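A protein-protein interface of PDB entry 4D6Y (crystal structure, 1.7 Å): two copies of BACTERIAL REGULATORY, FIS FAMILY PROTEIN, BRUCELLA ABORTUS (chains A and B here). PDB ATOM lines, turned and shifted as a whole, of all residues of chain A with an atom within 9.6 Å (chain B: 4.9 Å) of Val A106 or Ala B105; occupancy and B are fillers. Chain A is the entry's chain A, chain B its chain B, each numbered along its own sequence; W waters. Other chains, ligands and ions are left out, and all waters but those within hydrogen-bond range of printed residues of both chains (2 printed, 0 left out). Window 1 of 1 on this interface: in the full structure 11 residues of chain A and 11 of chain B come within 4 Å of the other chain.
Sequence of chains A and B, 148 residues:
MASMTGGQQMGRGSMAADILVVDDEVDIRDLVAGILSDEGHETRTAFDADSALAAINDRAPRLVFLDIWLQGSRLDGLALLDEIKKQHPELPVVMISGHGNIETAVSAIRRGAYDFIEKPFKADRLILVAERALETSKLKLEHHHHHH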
ATOM      1  N   ILE A  68      -3.281 -19.254 -29.991  1.00  0.00           N
ATOM      2  CA  ILE A  68      -3.293 -17.919 -30.599  1.00  0.00           C
ATOM      3  C   ILE A  68      -4.571 -17.739 -31.411  1.00  0.00           C
ATOM      4  O   ILE A  68      -5.310 -16.777 -31.170  1.00  0.00           O
ATOM      5  CB  ILE A  68      -2.008 -17.662 -31.432  1.00  0.00           C
ATOM      6  CG1 ILE A  68      -0.792 -17.580 -30.492  1.00  0.00           C
ATOM      7  CG2 ILE A  68      -2.124 -16.406 -32.276  1.00  0.00           C
ATOM      8  CD1 ILE A  68       0.584 -17.614 -31.190  1.00  0.00           C
ATOM      9  N   LEU A  78      -2.733 -13.505 -28.637  1.00  0.00           N
ATOM     10  CA  LEU A  78      -1.674 -12.532 -28.340  1.00  0.00           C
ATOM     11  C   LEU A  78      -2.259 -11.292 -27.637  1.00  0.00           C
ATOM     12  O   LEU A  78      -1.655 -10.789 -26.691  1.00  0.00           O
ATOM     13  CB  LEU A  78      -0.873 -12.155 -29.582  1.00  0.00           C
ATOM     14  CG  LEU A  78      -0.030 -13.271 -30.183  1.00  0.00           C
ATOM     15  CD1 LEU A  78       0.294 -12.982 -31.639  1.00  0.00           C
ATOM     16  CD2 LEU A  78       1.199 -13.521 -29.361  1.00  0.00           C
ATOM     17  N   LEU A  81      -2.922 -12.479 -24.201  1.00  0.00           N
ATOM     18  CA  LEU A  81      -1.639 -12.463 -23.469  1.00  0.00           C
ATOM     19  C   LEU A  81      -1.388 -11.064 -22.911  1.00  0.00           C
ATOM     20  O   LEU A  81      -1.067 -10.917 -21.738  1.00  0.00           O
ATOM     21  CB  LEU A  81      -0.495 -12.864 -24.417  1.00  0.00           C
ATOM     22  CG  LEU A  81       0.929 -12.639 -23.894  1.00  0.00           C
ATOM     23  CD1 LEU A  81       1.238 -13.583 -22.712  1.00  0.00           C
ATOM     24  CD2 LEU A  81       1.942 -12.821 -25.026  1.00  0.00           C
ATOM     25  N   MET A  95       2.633 -19.869 -24.713  1.00  0.00           N
ATOM     26  CA  MET A  95       1.818 -20.012 -25.908  1.00  0.00           C
ATOM     27  C   MET A  95       1.877 -21.442 -26.403  1.00  0.00           C
ATOM     28  O   MET A  95       2.936 -22.074 -26.334  1.00  0.00           O
ATOM     29  CB  MET A  95       2.296 -19.063 -27.038  1.00  0.00           C
ATOM     30  CG  MET A  95       2.445 -17.597 -26.615  1.00  0.00           C
ATOM     31  SD  MET A  95       1.044 -16.922 -25.709  1.00  0.00           S
ATOM     32  CE  MET A  95      -0.229 -16.902 -26.960  1.00  0.00           C
ATOM     33  N   GLY A 100       2.336 -20.379 -35.302  1.00  0.00           N
ATOM     34  CA  GLY A 100       3.536 -19.606 -35.043  1.00  0.00           C
ATOM     35  C   GLY A 100       4.450 -19.489 -36.236  1.00  0.00           C
ATOM     36  O   GLY A 100       4.352 -20.240 -37.209  1.00  0.00           O
ATOM     37  N   ASN A 101       5.341 -18.501 -36.153  1.00  0.00           N
ATOM     38  CA  ASN A 101       6.470 -18.272 -37.051  1.00  0.00           C
ATOM     39  C   ASN A 101       7.411 -17.478 -36.197  1.00  0.00           C
ATOM     40  O   ASN A 101       7.068 -17.230 -35.039  1.00  0.00           O
ATOM     41  CB  ASN A 101       6.078 -17.603 -38.375  1.00  0.00           C
ATOM     42  CG  ASN A 101       5.198 -16.384 -38.265  1.00  0.00           C
ATOM     43  OD1 ASN A 101       4.252 -16.208 -39.037  1.00  0.00           O
ATOM     44  ND2 ASN A 101       5.484 -15.511 -37.316  1.00  0.00           N
ATOM     45  N   ILE A 102       8.599 -17.179 -36.687  1.00  0.00           N
ATOM     46  CA  ILE A 102       9.590 -16.455 -35.895  1.00  0.00           C
ATOM     47  C   ILE A 102       9.025 -15.113 -35.402  1.00  0.00           C
ATOM     48  O   ILE A 102       9.148 -14.830 -34.207  1.00  0.00           O
ATOM     49  CB  ILE A 102      10.911 -16.308 -36.697  1.00  0.00           C
ATOM     50  CG1 ILE A 102      11.635 -17.677 -36.780  1.00  0.00           C
ATOM     51  CG2 ILE A 102      11.845 -15.198 -36.118  1.00  0.00           C
ATOM     52  CD1 ILE A 102      12.835 -17.705 -37.687  1.00  0.00           C
ATOM     53  N   GLU A 103       8.406 -14.307 -36.292  1.00  0.00           N
ATOM     54  CA  GLU A 103       7.903 -12.985 -35.900  1.00  0.00           C
ATOM     55  C   GLU A 103       6.849 -13.110 -34.799  1.00  0.00           C
ATOM     56  O   GLU A 103       6.874 -12.335 -33.851  1.00  0.00           O
ATOM     57  CB  GLU A 103       7.320 -12.232 -37.116  1.00  0.00           C
ATOM     58  CG  GLU A 103       7.040 -10.765 -36.810  1.00  0.00           C
ATOM     59  CD  GLU A 103       6.582  -9.882 -37.956  1.00  0.00           C
ATOM     60  OE1 GLU A 103       6.266 -10.411 -39.046  1.00  0.00           O
ATOM     61  OE2 GLU A 103       6.520  -8.649 -37.748  1.00  0.00           O
ATOM     62  N   THR A 104       5.954 -14.120 -34.898  1.00  0.00           N
ATOM     63  CA  THR A 104       4.876 -14.318 -33.920  1.00  0.00           C
ATOM     64  C   THR A 104       5.444 -14.766 -32.573  1.00  0.00           C
ATOM     65  O   THR A 104       5.039 -14.237 -31.530  1.00  0.00           O
ATOM     66  CB  THR A 104       3.851 -15.313 -34.489  1.00  0.00           C
ATOM     67  OG1 THR A 104       3.337 -14.759 -35.713  1.00  0.00           O
ATOM     68  CG2 THR A 104       2.693 -15.601 -33.516  1.00  0.00           C
ATOM     69  N   ALA A 105       6.420 -15.711 -32.593  1.00  0.00           N
ATOM     70  CA  ALA A 105       7.039 -16.192 -31.353  1.00  0.00           C
ATOM     71  C   ALA A 105       7.814 -15.061 -30.653  1.00  0.00           C
ATOM     72  O   ALA A 105       7.645 -14.882 -29.452  1.00  0.00           O
ATOM     73  CB  ALA A 105       7.950 -17.368 -31.638  1.00  0.00           C
ATOM     74  N   VAL A 106       8.593 -14.253 -31.410  1.00  0.00           N
ATOM     75  CA  VAL A 106       9.334 -13.114 -30.854  1.00  0.00           C
ATOM     76  C   VAL A 106       8.354 -12.164 -30.203  1.00  0.00           C
ATOM     77  O   VAL A 106       8.569 -11.756 -29.071  1.00  0.00           O
ATOM     78  CB  VAL A 106      10.203 -12.399 -31.924  1.00  0.00           C
ATOM     79  CG1 VAL A 106      10.711 -11.037 -31.420  1.00  0.00           C
ATOM     80  CG2 VAL A 106      11.356 -13.298 -32.362  1.00  0.00           C
ATOM     81  N   SER A 107       7.251 -11.851 -30.906  1.00  0.00           N
ATOM     82  CA  SER A 107       6.228 -10.960 -30.396  1.00  0.00           C
ATOM     83  C   SER A 107       5.667 -11.491 -29.090  1.00  0.00           C
ATOM     84  O   SER A 107       5.598 -10.723 -28.119  1.00  0.00           O
ATOM     85  CB  SER A 107       5.131 -10.764 -31.437  1.00  0.00           C
ATOM     86  OG  SER A 107       4.194  -9.818 -30.956  1.00  0.00           O
ATOM     87  N   ALA A 108       5.354 -12.815 -29.013  1.00  0.00           N
ATOM     88  CA  ALA A 108       4.804 -13.404 -27.787  1.00  0.00           C
ATOM     89  C   ALA A 108       5.783 -13.251 -26.625  1.00  0.00           C
ATOM     90  O   ALA A 108       5.383 -12.819 -25.544  1.00  0.00           O
ATOM     91  CB  ALA A 108       4.498 -14.864 -28.021  1.00  0.00           C
ATOM     92  N   ILE A 109       7.071 -13.559 -26.841  1.00  0.00           N
ATOM     93  CA  ILE A 109       8.026 -13.445 -25.719  1.00  0.00           C
ATOM     94  C   ILE A 109       8.197 -11.978 -25.315  1.00  0.00           C
ATOM     95  O   ILE A 109       8.217 -11.671 -24.112  1.00  0.00           O
ATOM     96  CB  ILE A 109       9.399 -14.105 -26.030  1.00  0.00           C
ATOM     97  CG1 ILE A 109       9.229 -15.540 -26.588  1.00  0.00           C
ATOM     98  CG2 ILE A 109      10.326 -14.063 -24.795  1.00  0.00           C
ATOM     99  CD1 ILE A 109       8.398 -16.584 -25.681  1.00  0.00           C
ATOM    100  N   ARG A 110       8.278 -11.068 -26.296  1.00  0.00           N
ATOM    101  CA  ARG A 110       8.442  -9.643 -25.960  1.00  0.00           C
ATOM    102  C   ARG A 110       7.249  -9.099 -25.176  1.00  0.00           C
ATOM    103  O   ARG A 110       7.402  -8.189 -24.333  1.00  0.00           O
ATOM    104  CB  ARG A 110       8.605  -8.807 -27.235  1.00  0.00           C
ATOM    105  CG  ARG A 110      10.004  -8.845 -27.839  1.00  0.00           C
ATOM    106  CD  ARG A 110      10.299  -7.454 -28.362  1.00  0.00           C
ATOM    107  NE  ARG A 110       9.530  -7.192 -29.574  1.00  0.00           N
ATOM    108  CZ  ARG A 110      10.014  -6.553 -30.632  1.00  0.00           C
ATOM    109  NH1 ARG A 110      11.256  -6.086 -30.622  1.00  0.00           N
ATOM    110  NH2 ARG A 110       9.258  -6.366 -31.706  1.00  0.00           N
ATOM    111  N   ARG A 111       6.065  -9.664 -25.441  1.00  0.00           N
ATOM    112  CA  ARG A 111       4.803  -9.262 -24.802  1.00  0.00           C
ATOM    113  C   ARG A 111       4.578  -9.977 -23.461  1.00  0.00           C
ATOM    114  O   ARG A 111       3.555  -9.730 -22.821  1.00  0.00           O
ATOM    115  CB  ARG A 111       3.627  -9.469 -25.773  1.00  0.00           C
ATOM    116  CG  ARG A 111       3.668  -8.354 -26.829  1.00  0.00           C
ATOM    117  CD  ARG A 111       3.011  -8.767 -28.118  1.00  0.00           C
ATOM    118  NE  ARG A 111       1.562  -8.632 -28.065  1.00  0.00           N
ATOM    119  CZ  ARG A 111       0.775  -8.781 -29.122  1.00  0.00           C
ATOM    120  NH1 ARG A 111       1.292  -9.101 -30.302  1.00  0.00           N
ATOM    121  NH2 ARG A 111      -0.537  -8.647 -29.004  1.00  0.00           N
ATOM    122  N   GLY A 112       5.556 -10.777 -23.023  1.00  0.00           N
ATOM    123  CA  GLY A 112       5.518 -11.404 -21.709  1.00  0.00           C
ATOM    124  C   GLY A 112       5.358 -12.901 -21.608  1.00  0.00           C
ATOM    125  O   GLY A 112       5.392 -13.434 -20.491  1.00  0.00           O
ATOM    126  N   ALA A 113       5.177 -13.616 -22.741  1.00  0.00           N
ATOM    127  CA  ALA A 113       5.080 -15.078 -22.651  1.00  0.00           C
ATOM    128  C   ALA A 113       6.393 -15.668 -22.197  1.00  0.00           C
ATOM    129  O   ALA A 113       7.468 -15.179 -22.561  1.00  0.00           O
ATOM    130  CB  ALA A 113       4.688 -15.700 -23.987  1.00  0.00           C
ATOM    131  N   TYR A 114       6.304 -16.705 -21.387  1.00  0.00           N
ATOM    132  CA  TYR A 114       7.434 -17.401 -20.825  1.00  0.00           C
ATOM    133  C   TYR A 114       8.132 -18.234 -21.881  1.00  0.00           C
ATOM    134  O   TYR A 114       9.365 -18.354 -21.886  1.00  0.00           O
ATOM    135  CB  TYR A 114       6.946 -18.292 -19.666  1.00  0.00           C
ATOM    136  CG  TYR A 114       8.057 -19.070 -19.015  1.00  0.00           C
ATOM    137  CD1 TYR A 114       8.932 -18.457 -18.121  1.00  0.00           C
ATOM    138  CD2 TYR A 114       8.243 -20.422 -19.289  1.00  0.00           C
ATOM    139  CE1 TYR A 114       9.997 -19.154 -17.560  1.00  0.00           C
ATOM    140  CE2 TYR A 114       9.302 -21.129 -18.731  1.00  0.00           C
ATOM    141  CZ  TYR A 114      10.167 -20.493 -17.853  1.00  0.00           C
ATOM    142  OH  TYR A 114      11.203 -21.187 -17.276  1.00  0.00           O
ATOM    143  N   ASP A 115       7.320 -18.902 -22.709  1.00  0.00           N
ATOM    144  CA  ASP A 115       7.799 -19.784 -23.747  1.00  0.00           C
ATOM    145  C   ASP A 115       6.710 -19.962 -24.819  1.00  0.00           C
ATOM    146  O   ASP A 115       5.590 -19.466 -24.691  1.00  0.00           O
ATOM    147  CB  ASP A 115       8.221 -21.142 -23.123  1.00  0.00           C
ATOM    148  CG  ASP A 115       9.260 -21.954 -23.888  1.00  0.00           C
ATOM    149  OD1 ASP A 115       9.526 -21.631 -25.079  1.00  0.00           O
ATOM    150  OD2 ASP A 115       9.810 -22.919 -23.299  1.00  0.00           O
ATOM    151  N   PHE A 116       7.097 -20.609 -25.900  1.00  0.00           N
ATOM    152  CA  PHE A 116       6.245 -20.875 -27.042  1.00  0.00           C
ATOM    153  C   PHE A 116       6.355 -22.345 -27.394  1.00  0.00           C
ATOM    154  O   PHE A 116       7.457 -22.830 -27.690  1.00  0.00           O
ATOM    155  CB  PHE A 116       6.656 -19.977 -28.230  1.00  0.00           C
ATOM    156  CG  PHE A 116       5.619 -19.860 -29.319  1.00  0.00           C
ATOM    157  CD1 PHE A 116       5.385 -20.910 -30.195  1.00  0.00           C
ATOM    158  CD2 PHE A 116       4.921 -18.682 -29.506  1.00  0.00           C
ATOM    159  CE1 PHE A 116       4.438 -20.791 -31.215  1.00  0.00           C
ATOM    160  CE2 PHE A 116       3.970 -18.569 -30.519  1.00  0.00           C
ATOM    161  CZ  PHE A 116       3.724 -19.630 -31.357  1.00  0.00           C
ATOM    162  N   GLU A 118       5.271 -25.201 -30.014  1.00  0.00           N
ATOM    163  CA  GLU A 118       4.681 -25.420 -31.331  1.00  0.00           C
ATOM    164  C   GLU A 118       3.809 -26.657 -31.352  1.00  0.00           C
ATOM    165  O   GLU A 118       4.211 -27.716 -30.847  1.00  0.00           O
ATOM    166  CB  GLU A 118       5.776 -25.592 -32.403  1.00  0.00           C
ATOM    167  CG  GLU A 118       6.639 -24.368 -32.658  1.00  0.00           C
ATOM    168  CD  GLU A 118       7.819 -24.706 -33.553  1.00  0.00           C
ATOM    169  OE1 GLU A 118       7.604 -25.016 -34.747  1.00  0.00           O
ATOM    170  OE2 GLU A 118       8.957 -24.744 -33.037  1.00  0.00           O
ATOM    171  N   ASN B 101      14.662 -20.395 -36.271  1.00  0.00           N
ATOM    172  CA  ASN B 101      13.428 -21.171 -36.232  1.00  0.00           C
ATOM    173  C   ASN B 101      12.764 -20.669 -34.985  1.00  0.00           C
ATOM    174  O   ASN B 101      13.352 -19.815 -34.325  1.00  0.00           O
ATOM    175  CB  ASN B 101      13.639 -22.697 -36.286  1.00  0.00           C
ATOM    176  CG  ASN B 101      14.662 -23.247 -35.331  1.00  0.00           C
ATOM    177  OD1 ASN B 101      15.461 -24.117 -35.686  1.00  0.00           O
ATOM    178  ND2 ASN B 101      14.668 -22.757 -34.105  1.00  0.00           N
ATOM    179  N   ILE B 102      11.547 -21.108 -34.696  1.00  0.00           N
ATOM    180  CA  ILE B 102      10.822 -20.608 -33.523  1.00  0.00           C
ATOM    181  C   ILE B 102      11.622 -20.853 -32.244  1.00  0.00           C
ATOM    182  O   ILE B 102      11.772 -19.919 -31.452  1.00  0.00           O
ATOM    183  CB  ILE B 102       9.396 -21.201 -33.474  1.00  0.00           C
ATOM    184  CG1 ILE B 102       8.515 -20.591 -34.586  1.00  0.00           C
ATOM    185  CG2 ILE B 102       8.714 -21.028 -32.084  1.00  0.00           C
ATOM    186  CD1 ILE B 102       7.205 -21.372 -34.863  1.00  0.00           C
ATOM    187  N   GLU B 103      12.141 -22.080 -32.045  1.00  0.00           N
ATOM    188  CA  GLU B 103      12.869 -22.384 -30.803  1.00  0.00           C
ATOM    189  C   GLU B 103      14.107 -21.497 -30.640  1.00  0.00           C
ATOM    190  O   GLU B 103      14.360 -21.011 -29.539  1.00  0.00           O
ATOM    191  CB  GLU B 103      13.293 -23.867 -30.772  1.00  0.00           C
ATOM    192  CG  GLU B 103      13.724 -24.306 -29.379  1.00  0.00           C
ATOM    193  CD  GLU B 103      14.033 -25.778 -29.167  1.00  0.00           C
ATOM    194  OE1 GLU B 103      13.998 -26.553 -30.151  1.00  0.00           O
ATOM    195  OE2 GLU B 103      14.309 -26.155 -28.005  1.00  0.00           O
ATOM    196  N   THR B 104      14.838 -21.226 -31.746  1.00  0.00           N
ATOM    197  CA  THR B 104      16.054 -20.410 -31.700  1.00  0.00           C
ATOM    198  C   THR B 104      15.711 -18.951 -31.409  1.00  0.00           C
ATOM    199  O   THR B 104      16.376 -18.318 -30.569  1.00  0.00           O
ATOM    200  CB  THR B 104      16.831 -20.565 -33.031  1.00  0.00           C
ATOM    201  OG1 THR B 104      17.163 -21.944 -33.151  1.00  0.00           O
ATOM    202  CG2 THR B 104      18.117 -19.709 -33.085  1.00  0.00           C
ATOM    203  N   ALA B 105      14.643 -18.430 -32.061  1.00  0.00           N
ATOM    204  CA  ALA B 105      14.225 -17.038 -31.826  1.00  0.00           C
ATOM    205  C   ALA B 105      13.732 -16.849 -30.370  1.00  0.00           C
ATOM    206  O   ALA B 105      14.144 -15.894 -29.729  1.00  0.00           O
ATOM    207  CB  ALA B 105      13.139 -16.639 -32.804  1.00  0.00           C
ATOM    208  N   VAL B 106      12.939 -17.806 -29.835  1.00  0.00           N
ATOM    209  CA  VAL B 106      12.459 -17.742 -28.445  1.00  0.00           C
ATOM    210  C   VAL B 106      13.650 -17.720 -27.517  1.00  0.00           C
ATOM    211  O   VAL B 106      13.714 -16.884 -26.622  1.00  0.00           O
ATOM    212  CB  VAL B 106      11.495 -18.901 -28.098  1.00  0.00           C
ATOM    213  CG1 VAL B 106      11.242 -18.962 -26.587  1.00  0.00           C
ATOM    214  CG2 VAL B 106      10.178 -18.755 -28.860  1.00  0.00           C
ATOM    215  N   SER B 107      14.631 -18.615 -27.769  1.00  0.00           N
ATOM    216  CA  SER B 107      15.838 -18.672 -26.963  1.00  0.00           C
ATOM    217  C   SER B 107      16.571 -17.344 -26.980  1.00  0.00           C
ATOM    218  O   SER B 107      16.930 -16.845 -25.912  1.00  0.00           O
ATOM    219  CB  SER B 107      16.745 -19.800 -27.452  1.00  0.00           C
ATOM    220  OG  SER B 107      17.865 -19.894 -26.594  1.00  0.00           O
ATOM    221  N   ALA B 108      16.720 -16.704 -28.185  1.00  0.00           N
ATOM    222  CA  ALA B 108      17.410 -15.411 -28.280  1.00  0.00           C
ATOM    223  C   ALA B 108      16.704 -14.355 -27.448  1.00  0.00           C
ATOM    224  O   ALA B 108      17.365 -13.648 -26.674  1.00  0.00           O
ATOM    225  CB  ALA B 108      17.482 -14.975 -29.726  1.00  0.00           C
ATOM    226  N   ILE B 109      15.371 -14.263 -27.563  1.00  0.00           N
ATOM    227  CA  ILE B 109      14.664 -13.216 -26.782  1.00  0.00           C
ATOM    228  C   ILE B 109      14.763 -13.510 -25.273  1.00  0.00           C
ATOM    229  O   ILE B 109      14.997 -12.585 -24.481  1.00  0.00           O
ATOM    230  CB  ILE B 109      13.192 -13.030 -27.215  1.00  0.00           C
ATOM    231  CG1 ILE B 109      13.049 -12.886 -28.751  1.00  0.00           C
ATOM    232  CG2 ILE B 109      12.538 -11.857 -26.460  1.00  0.00           C
ATOM    233  CD1 ILE B 109      13.904 -11.704 -29.429  1.00  0.00           C
ATOM    234  N   ASP B 115      15.217  -8.164 -30.402  1.00  0.00           N
ATOM    235  CA  ASP B 115      14.439  -8.625 -31.535  1.00  0.00           C
ATOM    236  C   ASP B 115      15.275  -9.601 -32.371  1.00  0.00           C
ATOM    237  O   ASP B 115      16.467  -9.847 -32.103  1.00  0.00           O
ATOM    238  CB  ASP B 115      13.973  -7.402 -32.379  1.00  0.00           C
ATOM    239  CG  ASP B 115      12.697  -7.590 -33.203  1.00  0.00           C
ATOM    240  OD1 ASP B 115      12.267  -8.755 -33.385  1.00  0.00           O
ATOM    241  OD2 ASP B 115      12.117  -6.561 -33.654  1.00  0.00           O
ATOM    242  N   PHE B 116      14.606 -10.222 -33.327  1.00  0.00           N
ATOM    243  CA  PHE B 116      15.186 -11.191 -34.233  1.00  0.00           C
ATOM    244  C   PHE B 116      14.816 -10.815 -35.656  1.00  0.00           C
ATOM    245  O   PHE B 116      13.630 -10.735 -35.990  1.00  0.00           O
ATOM    246  CB  PHE B 116      14.691 -12.603 -33.872  1.00  0.00           C
ATOM    247  CG  PHE B 116      15.510 -13.732 -34.451  1.00  0.00           C
ATOM    248  CD1 PHE B 116      15.429 -14.050 -35.802  1.00  0.00           C
ATOM    249  CD2 PHE B 116      16.318 -14.509 -33.636  1.00  0.00           C
ATOM    250  CE1 PHE B 116      16.177 -15.107 -36.332  1.00  0.00           C
ATOM    251  CE2 PHE B 116      17.073 -15.556 -34.165  1.00  0.00           C
ATOM    252  CZ  PHE B 116      17.009 -15.839 -35.518  1.00  0.00           C
HETATM  253  O   HOH W   1      11.464 -24.368 -33.710  1.00  0.00           O
HETATM  254  O   HOH W   2       9.874  -5.580 -34.659  1.00  0.00           O
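Of the 11 printed residues of chain B, 7 touch a printed residue of chain A.
Printed residues of chain B that touch a printed residue of chain A: Asn B101, Ile B102, Ala B105, Val B106, Ile B109, Asp B115 and Phe B116.
Hydrophobic or aromatic side chains of chain B that line the printed part of chain A: Ile B102, Ala B105, Val B106, Ile B109 and Phe B116.
Of the 22 printed residues of chain A, 10 touch a printed residue of chain B.
Hydrophobic or aromatic side chains of chain A that line the printed part of chain B: Ile A102, Ala A105, Val A106, Ile A109 and Phe A116.
Along chain A the printed residues that touch a printed residue of chain B span positions 100 to 118.
Among the printed residues, 18 pairs touch across the chains.
Among the printed residues, Asp or Glu carboxylates within 4 Å of a Lys or Arg side-chain nitrogen of the other chain: Arg A110 with Asp B115 (3.2 Å).
Ala A105 touches Val B106, and with the chains exchanged Val A106 touches Ala B105.
Val A106 touches Ile B109, and with the chains exchanged Ile A109 touches Val B106.
Val A106 touches Asp B115, and with the chains exchanged Asp A115 touches Val B106.
Ile A109 touches its own counterpart, Ile B109.
Positions printed for both chains: 101, 102, 103, 104, 105, 106, 107, 108, 109, 115 and 116.
The guanidinium group (NH1) of Arg A110 is in salt-bridge range of the side-chain carboxylate (OD2) of Asp B115, at 3.2 Å.
The backbone NH (N) of Met A95 sits at hydrogen-bond distance from the backbone carbonyl oxygen (O) of Asp A115 (3.0 Å).
OG1 of Thr B104 sits at hydrogen-bond distance from ND2 of Asn B101, 2.8 Å away.
ND2 of Asn A101 lies close to N of Glu A103 (3.3 Å).
ND2 of Asn B101 sits close to N of Glu B103.
OG1 of Thr A104 is in hydrogen-bond range of ND2 of Asn A101 (2.8 Å).
Val A106 touches just these residues of chain B: Ala B105, Ile B109, Asp B115 and Phe B116.
Ala B105 touches just these residues of chain A: Ile A102 and Val A106.
No residue of chain A comes within 4 Å of Thr B104.
Val B106 touches just these residues of chain A: Ala A105, Ile A109, Asp A115 and Phe A116.
No residue of chain A comes within 4 Å of Ala B108.
Of the printed residues of chain A, Asp B115 touches Val A106 and Arg A110.
Printed residues of chain B within 4 Å of Asn A101: Ile B102.
Ser A107 touches none of the printed residues of chain B.
Tyr A114 touches none of the printed residues of chain B.
The nearest printed residue of chain B that does not touch Val A106 is Val B106 (5.4 Å).
Among the printed residues, merely in contact across the chains: Val A106 with Asp B115 (3.4 Å), Asp A115 with Val B106 (3.5 Å), Ile A109 with Ile B109 (3.5 Å), Ile A102 with Asn B101 (3.5 Å), Glu A118 with Ile B102 (3.6 Å), Gly A100 with Ile B102 (3.6 Å), Asn A101 with Ile B102 (3.7 Å), Val A106 with Phe B116 (3.7 Å), Ala A105 with Ile B102 (3.8 Å), Ile A102 with Phe B116 (3.8 Å), Phe A116 with Val B106 (3.8 Å), Val A106 with Ala B105 (3.8 Å), Ile A109 with Val B106 (3.8 Å), Val A106 with Ile B109 (3.8 Å), Ala A105 with Val B106 (3.8 Å), Phe A116 with Ile B102 (3.8 Å) and Ile A102 with Ala B105 (3.8 Å).
Water W1 lies within hydrogen-bond range of OE2 of Glu A118, N of Glu B103 and N of Ile B102.
Water W2 lies within hydrogen-bond range of OD2 of Asp B115 (2.6 Å) and NH2 of Arg A110 (3.1 Å).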
